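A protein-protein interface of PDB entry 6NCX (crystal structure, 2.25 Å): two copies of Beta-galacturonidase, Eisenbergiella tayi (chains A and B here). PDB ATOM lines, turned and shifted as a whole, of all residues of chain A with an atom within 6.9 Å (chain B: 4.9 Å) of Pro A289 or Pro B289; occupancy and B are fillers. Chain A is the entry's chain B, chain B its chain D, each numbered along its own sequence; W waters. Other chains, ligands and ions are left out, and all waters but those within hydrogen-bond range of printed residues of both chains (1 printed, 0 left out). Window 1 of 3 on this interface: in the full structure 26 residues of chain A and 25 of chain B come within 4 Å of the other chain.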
ATOM      1  N   PRO A  40     -24.545  29.914   4.130  1.00  0.00           N
ATOM      2  CA  PRO A  40     -25.786  29.763   4.917  1.00  0.00           C
ATOM      3  C   PRO A  40     -25.693  30.304   6.356  1.00  0.00           C
ATOM      4  O   PRO A  40     -24.583  30.495   6.880  1.00  0.00           O
ATOM      5  CB  PRO A  40     -26.023  28.238   4.930  1.00  0.00           C
ATOM      6  CG  PRO A  40     -24.662  27.647   4.692  1.00  0.00           C
ATOM      7  CD  PRO A  40     -23.942  28.614   3.786  1.00  0.00           C
ATOM      8  N   HIS A 281     -29.528  23.632  16.464  1.00  0.00           N
ATOM      9  CA  HIS A 281     -28.244  23.762  17.126  1.00  0.00           C
ATOM     10  C   HIS A 281     -28.209  25.176  17.671  1.00  0.00           C
ATOM     11  O   HIS A 281     -28.679  26.090  16.986  1.00  0.00           O
ATOM     12  CB  HIS A 281     -27.077  23.520  16.169  1.00  0.00           C
ATOM     13  CG  HIS A 281     -25.726  23.527  16.818  1.00  0.00           C
ATOM     14  ND1 HIS A 281     -25.100  24.684  17.232  1.00  0.00           N
ATOM     15  CD2 HIS A 281     -24.861  22.516  17.090  1.00  0.00           C
ATOM     16  CE1 HIS A 281     -23.921  24.384  17.757  1.00  0.00           C
ATOM     17  NE2 HIS A 281     -23.751  23.074  17.682  1.00  0.00           N
ATOM     18  N   PHE A 284     -26.151  27.540  15.297  1.00  0.00           N
ATOM     19  CA  PHE A 284     -26.332  27.467  13.860  1.00  0.00           C
ATOM     20  C   PHE A 284     -27.798  27.480  13.451  1.00  0.00           C
ATOM     21  O   PHE A 284     -28.094  27.432  12.245  1.00  0.00           O
ATOM     22  CB  PHE A 284     -25.642  26.206  13.329  1.00  0.00           C
ATOM     23  CG  PHE A 284     -24.191  26.101  13.713  1.00  0.00           C
ATOM     24  CD1 PHE A 284     -23.338  27.200  13.591  1.00  0.00           C
ATOM     25  CD2 PHE A 284     -23.665  24.892  14.182  1.00  0.00           C
ATOM     26  CE1 PHE A 284     -21.970  27.096  13.928  1.00  0.00           C
ATOM     27  CE2 PHE A 284     -22.313  24.781  14.523  1.00  0.00           C
ATOM     28  CZ  PHE A 284     -21.462  25.889  14.395  1.00  0.00           C
ATOM     29  N   CYS A 286     -31.034  26.278  12.202  1.00  0.00           N
ATOM     30  CA  CYS A 286     -31.201  25.141  11.301  1.00  0.00           C
ATOM     31  C   CYS A 286     -30.214  25.195  10.129  1.00  0.00           C
ATOM     32  O   CYS A 286     -30.337  24.402   9.187  1.00  0.00           O
ATOM     33  CB  CYS A 286     -32.649  25.053  10.800  1.00  0.00           C
ATOM     34  SG  CYS A 286     -33.134  26.448   9.794  1.00  0.00           S
ATOM     35  N   ALA A 287     -29.236  26.098  10.173  1.00  0.00           N
ATOM     36  CA  ALA A 287     -28.142  26.128   9.197  1.00  0.00           C
ATOM     37  C   ALA A 287     -26.886  25.449   9.759  1.00  0.00           C
ATOM     38  O   ALA A 287     -25.832  26.075   9.955  1.00  0.00           O
ATOM     39  CB  ALA A 287     -27.847  27.565   8.784  1.00  0.00           C
ATOM     40  N   LEU A 288     -27.001  24.150  10.022  1.00  0.00           N
ATOM     41  CA  LEU A 288     -25.890  23.427  10.635  1.00  0.00           C
ATOM     42  C   LEU A 288     -24.858  23.083   9.565  1.00  0.00           C
ATOM     43  O   LEU A 288     -25.228  22.586   8.494  1.00  0.00           O
ATOM     44  CB  LEU A 288     -26.371  22.142  11.347  1.00  0.00           C
ATOM     45  CG  LEU A 288     -26.912  22.220  12.792  1.00  0.00           C
ATOM     46  CD1 LEU A 288     -28.234  22.957  12.810  1.00  0.00           C
ATOM     47  CD2 LEU A 288     -27.064  20.830  13.484  1.00  0.00           C
ATOM     48  N   PRO A 289     -23.572  23.331   9.815  1.00  0.00           N
ATOM     49  CA  PRO A 289     -22.536  22.946   8.854  1.00  0.00           C
ATOM     50  C   PRO A 289     -22.252  21.449   8.864  1.00  0.00           C
ATOM     51  O   PRO A 289     -22.599  20.719   9.792  1.00  0.00           O
ATOM     52  CB  PRO A 289     -21.311  23.734   9.331  1.00  0.00           C
ATOM     53  CG  PRO A 289     -21.520  23.863  10.787  1.00  0.00           C
ATOM     54  CD  PRO A 289     -23.007  24.089  10.949  1.00  0.00           C
ATOM     55  N   PHE A 290     -21.613  21.013   7.775  1.00  0.00           N
ATOM     56  CA  PHE A 290     -21.094  19.655   7.615  1.00  0.00           C
ATOM     57  C   PHE A 290     -20.477  19.080   8.896  1.00  0.00           C
ATOM     58  O   PHE A 290     -20.798  17.953   9.301  1.00  0.00           O
ATOM     59  CB  PHE A 290     -20.070  19.678   6.462  1.00  0.00           C
ATOM     60  CG  PHE A 290     -19.154  18.494   6.432  1.00  0.00           C
ATOM     61  CD1 PHE A 290     -19.605  17.263   5.964  1.00  0.00           C
ATOM     62  CD2 PHE A 290     -17.841  18.610   6.871  1.00  0.00           C
ATOM     63  CE1 PHE A 290     -18.769  16.169   5.943  1.00  0.00           C
ATOM     64  CE2 PHE A 290     -16.991  17.519   6.856  1.00  0.00           C
ATOM     65  CZ  PHE A 290     -17.453  16.292   6.387  1.00  0.00           C
ATOM     66  N   SER A 291     -19.591  19.846   9.547  1.00  0.00           N
ATOM     67  CA  SER A 291     -18.963  19.393  10.791  1.00  0.00           C
ATOM     68  C   SER A 291     -19.992  19.175  11.905  1.00  0.00           C
ATOM     69  O   SER A 291     -19.869  18.232  12.697  1.00  0.00           O
ATOM     70  CB  SER A 291     -17.904  20.405  11.251  1.00  0.00           C
ATOM     71  OG  SER A 291     -16.775  20.457  10.393  1.00  0.00           O
ATOM     72  N   ALA A 292     -20.998  20.052  12.009  1.00  0.00           N
ATOM     73  CA  ALA A 292     -22.025  19.849  13.031  1.00  0.00           C
ATOM     74  C   ALA A 292     -22.935  18.674  12.681  1.00  0.00           C
ATOM     75  O   ALA A 292     -23.353  17.925  13.565  1.00  0.00           O
ATOM     76  CB  ALA A 292     -22.836  21.129  13.240  1.00  0.00           C
ATOM     77  N   MET A 293     -23.215  18.471  11.400  1.00  0.00           N
ATOM     78  CA  MET A 293     -23.984  17.304  10.984  1.00  0.00           C
ATOM     79  C   MET A 293     -23.263  16.014  11.344  1.00  0.00           C
ATOM     80  O   MET A 293     -23.835  15.126  11.989  1.00  0.00           O
ATOM     81  CB  MET A 293     -24.228  17.344   9.479  1.00  0.00           C
ATOM     82  CG  MET A 293     -25.262  18.327   9.008  1.00  0.00           C
ATOM     83  SD  MET A 293     -25.360  18.184   7.206  1.00  0.00           S
ATOM     84  CE  MET A 293     -26.377  19.605   6.839  1.00  0.00           C
ATOM     85  N   GLN A 294     -22.008  15.886  10.910  1.00  0.00           N
ATOM     86  CA  GLN A 294     -21.278  14.656  11.175  1.00  0.00           C
ATOM     87  C   GLN A 294     -21.086  14.424  12.671  1.00  0.00           C
ATOM     88  O   GLN A 294     -21.118  13.272  13.128  1.00  0.00           O
ATOM     89  CB  GLN A 294     -19.933  14.666  10.444  1.00  0.00           C
ATOM     90  CG  GLN A 294     -19.112  13.387  10.642  1.00  0.00           C
ATOM     91  CD  GLN A 294     -19.856  12.130  10.224  1.00  0.00           C
ATOM     92  OE1 GLN A 294     -20.843  12.196   9.496  1.00  0.00           O
ATOM     93  NE2 GLN A 294     -19.379  10.970  10.684  1.00  0.00           N
ATOM     94  N   HIS A 295     -20.914  15.497  13.454  1.00  0.00           N
ATOM     95  CA  HIS A 295     -20.805  15.320  14.898  1.00  0.00           C
ATOM     96  C   HIS A 295     -22.076  14.700  15.466  1.00  0.00           C
ATOM     97  O   HIS A 295     -22.003  13.787  16.304  1.00  0.00           O
ATOM     98  CB  HIS A 295     -20.487  16.654  15.574  1.00  0.00           C
ATOM     99  CG  HIS A 295     -19.967  16.510  16.969  1.00  0.00           C
ATOM    100  ND1 HIS A 295     -20.754  16.713  18.083  1.00  0.00           N
ATOM    101  CD2 HIS A 295     -18.744  16.159  17.432  1.00  0.00           C
ATOM    102  CE1 HIS A 295     -20.038  16.498  19.170  1.00  0.00           C
ATOM    103  NE2 HIS A 295     -18.816  16.158  18.804  1.00  0.00           N
ATOM    104  N   LEU A 318     -27.179  17.591   2.031  1.00  0.00           N
ATOM    105  CA  LEU A 318     -25.864  17.216   2.539  1.00  0.00           C
ATOM    106  C   LEU A 318     -25.995  16.160   3.631  1.00  0.00           C
ATOM    107  O   LEU A 318     -25.266  15.161   3.637  1.00  0.00           O
ATOM    108  CB  LEU A 318     -25.139  18.465   3.051  1.00  0.00           C
ATOM    109  CG  LEU A 318     -23.697  18.324   3.547  1.00  0.00           C
ATOM    110  CD1 LEU A 318     -22.800  17.691   2.510  1.00  0.00           C
ATOM    111  CD2 LEU A 318     -23.149  19.684   3.927  1.00  0.00           C
ATOM    112  N   LEU A 322     -24.771  12.156   3.829  1.00  0.00           N
ATOM    113  CA  LEU A 322     -23.956  11.560   4.878  1.00  0.00           C
ATOM    114  C   LEU A 322     -24.574  10.266   5.389  1.00  0.00           C
ATOM    115  O   LEU A 322     -23.843   9.347   5.789  1.00  0.00           O
ATOM    116  CB  LEU A 322     -23.759  12.571   6.014  1.00  0.00           C
ATOM    117  CG  LEU A 322     -22.789  13.704   5.656  1.00  0.00           C
ATOM    118  CD1 LEU A 322     -22.843  14.793   6.705  1.00  0.00           C
ATOM    119  CD2 LEU A 322     -21.390  13.129   5.507  1.00  0.00           C
ATOM    120  N   PHE B 284     -15.507  20.854  17.855  1.00  0.00           N
ATOM    121  CA  PHE B 284     -14.720  20.875  16.638  1.00  0.00           C
ATOM    122  C   PHE B 284     -13.224  20.823  16.901  1.00  0.00           C
ATOM    123  O   PHE B 284     -12.441  20.773  15.935  1.00  0.00           O
ATOM    124  CB  PHE B 284     -15.091  22.118  15.822  1.00  0.00           C
ATOM    125  CG  PHE B 284     -16.568  22.204  15.508  1.00  0.00           C
ATOM    126  CD1 PHE B 284     -17.262  21.078  15.043  1.00  0.00           C
ATOM    127  CD2 PHE B 284     -17.268  23.390  15.701  1.00  0.00           C
ATOM    128  CE1 PHE B 284     -18.626  21.124  14.756  1.00  0.00           C
ATOM    129  CE2 PHE B 284     -18.627  23.460  15.414  1.00  0.00           C
ATOM    130  CZ  PHE B 284     -19.313  22.310  14.939  1.00  0.00           C
ATOM    131  N   ALA B 287     -10.542  22.249  14.670  1.00  0.00           N
ATOM    132  CA  ALA B 287     -10.977  22.142  13.270  1.00  0.00           C
ATOM    133  C   ALA B 287     -12.344  22.797  13.080  1.00  0.00           C
ATOM    134  O   ALA B 287     -13.343  22.151  12.770  1.00  0.00           O
ATOM    135  CB  ALA B 287     -11.010  20.681  12.835  1.00  0.00           C
ATOM    136  N   LEU B 288     -12.369  24.104  13.247  1.00  0.00           N
ATOM    137  CA  LEU B 288     -13.652  24.804  13.266  1.00  0.00           C
ATOM    138  C   LEU B 288     -14.120  25.093  11.847  1.00  0.00           C
ATOM    139  O   LEU B 288     -13.338  25.589  11.037  1.00  0.00           O
ATOM    140  CB  LEU B 288     -13.552  26.111  14.051  1.00  0.00           C
ATOM    141  CG  LEU B 288     -13.593  26.009  15.561  1.00  0.00           C
ATOM    142  CD1 LEU B 288     -12.262  25.502  16.092  1.00  0.00           C
ATOM    143  CD2 LEU B 288     -13.907  27.367  16.126  1.00  0.00           C
ATOM    144  N   PRO B 289     -15.378  24.811  11.515  1.00  0.00           N
ATOM    145  CA  PRO B 289     -15.875  25.106  10.171  1.00  0.00           C
ATOM    146  C   PRO B 289     -16.105  26.600  10.008  1.00  0.00           C
ATOM    147  O   PRO B 289     -16.114  27.363  10.971  1.00  0.00           O
ATOM    148  CB  PRO B 289     -17.195  24.332  10.105  1.00  0.00           C
ATOM    149  CG  PRO B 289     -17.701  24.371  11.529  1.00  0.00           C
ATOM    150  CD  PRO B 289     -16.439  24.265  12.389  1.00  0.00           C
ATOM    151  N   PHE B 290     -16.280  27.000   8.751  1.00  0.00           N
ATOM    152  CA  PHE B 290     -16.657  28.358   8.361  1.00  0.00           C
ATOM    153  C   PHE B 290     -17.724  28.972   9.271  1.00  0.00           C
ATOM    154  O   PHE B 290     -17.598  30.128   9.693  1.00  0.00           O
ATOM    155  CB  PHE B 290     -17.152  28.338   6.905  1.00  0.00           C
ATOM    156  CG  PHE B 290     -17.841  29.606   6.470  1.00  0.00           C
ATOM    157  CD1 PHE B 290     -17.096  30.734   6.138  1.00  0.00           C
ATOM    158  CD2 PHE B 290     -19.230  29.675   6.396  1.00  0.00           C
ATOM    159  CE1 PHE B 290     -17.729  31.912   5.734  1.00  0.00           C
ATOM    160  CE2 PHE B 290     -19.869  30.849   5.989  1.00  0.00           C
ATOM    161  CZ  PHE B 290     -19.115  31.970   5.658  1.00  0.00           C
ATOM    162  N   SER B 291     -18.772  28.195   9.573  1.00  0.00           N
ATOM    163  CA  SER B 291     -19.912  28.691  10.344  1.00  0.00           C
ATOM    164  C   SER B 291     -19.525  29.033  11.783  1.00  0.00           C
ATOM    165  O   SER B 291     -19.979  30.040  12.342  1.00  0.00           O
ATOM    166  CB  SER B 291     -21.022  27.636  10.349  1.00  0.00           C
ATOM    167  OG  SER B 291     -21.825  27.653   9.181  1.00  0.00           O
ATOM    168  N   ALA B 292     -18.729  28.176  12.420  1.00  0.00           N
ATOM    169  CA  ALA B 292     -18.293  28.456  13.778  1.00  0.00           C
ATOM    170  C   ALA B 292     -17.381  29.683  13.824  1.00  0.00           C
ATOM    171  O   ALA B 292     -17.513  30.530  14.722  1.00  0.00           O
ATOM    172  CB  ALA B 292     -17.602  27.224  14.343  1.00  0.00           C
ATOM    173  N   MET B 293     -16.471  29.806  12.843  1.00  0.00           N
ATOM    174  CA  MET B 293     -15.538  30.930  12.811  1.00  0.00           C
ATOM    175  C   MET B 293     -16.279  32.242  12.692  1.00  0.00           C
ATOM    176  O   MET B 293     -15.964  33.215  13.391  1.00  0.00           O
ATOM    177  CB  MET B 293     -14.573  30.826  11.627  1.00  0.00           C
ATOM    178  CG  MET B 293     -13.728  29.611  11.521  1.00  0.00           C
ATOM    179  SD  MET B 293     -12.741  29.849  10.021  1.00  0.00           S
ATOM    180  CE  MET B 293     -11.669  28.410  10.114  1.00  0.00           C
HETATM  181  O   HOH W   1     -23.372  29.526   9.169  1.00  0.00           O
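Hydrophobic or aromatic side chains of chain B within 4 Å of the printed part of chain A: Phe B284 and Pro B289.
Hydrophobic or aromatic side chains of chain A within 4 Å of the printed part of chain B: Phe A284 and Pro A289.
Among the printed residues, 8 pairs touch across the chains.
Among the printed residues, no Asp or Glu carboxylate lies within 4 Å of a Lys or Arg side-chain nitrogen of the other chain.
Phe A284 touches Phe B284 (CZ to CE2, 3.9 Å).
Ser B291 touches Phe A284 (CB to CE1, 3.7 Å).
Phe A284 touches Ala B292 (CE1 to N, 3.7 Å).
Pro B289 touches Pro A289 (CG to CG, 3.9 Å).
CB of Ser B291 touches CG of Pro A289, 3.8 Å away.
CE1 of Phe B284 touches CB of Ser A291, 3.7 Å away.
Pro B289 touches Ser A291 (CB to OG, 3.9 Å).
Phe B284 touches Ala A292.
Phe A284 touches its own counterpart, Phe B284.
Phe A284 touches Ser B291, and with the chains exchanged Ser A291 touches Phe B284.
Phe A284 touches Ala B292, and with the chains exchanged Ala A292 touches Phe B284.
Pro A289 touches Ser B291, and with the chains exchanged Ser A291 touches Pro B289.
8 positions are printed for both chains.
Of the 8 pairs that touch across the chains among the printed residues, 8 have their exchanged pair printed and touching as well.
Water W1 bridges the side-chain hydroxyl (OG) of Ser B291 (2.4 Å) and the backbone carbonyl oxygen (O) of Pro A40 (2.8 Å).
His A281 touches none of the printed residues of chain B.
Pro A289 touches just these residues of chain B: Pro B289 (3.9 Å) and Ser B291 (3.8 Å).
Of the printed residues of chain B, Ala A292 touches Phe B284 (3.8 Å).
Leu A318 touches none of the printed residues of chain B.
Of the printed residues of chain A, Phe B284 touches Phe A284 (3.9 Å), Ser A291 (3.7 Å) and Ala A292 (3.8 Å).
The nearest printed residue of chain B that does not touch Pro A289 is Phe B284 (5.0 Å).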
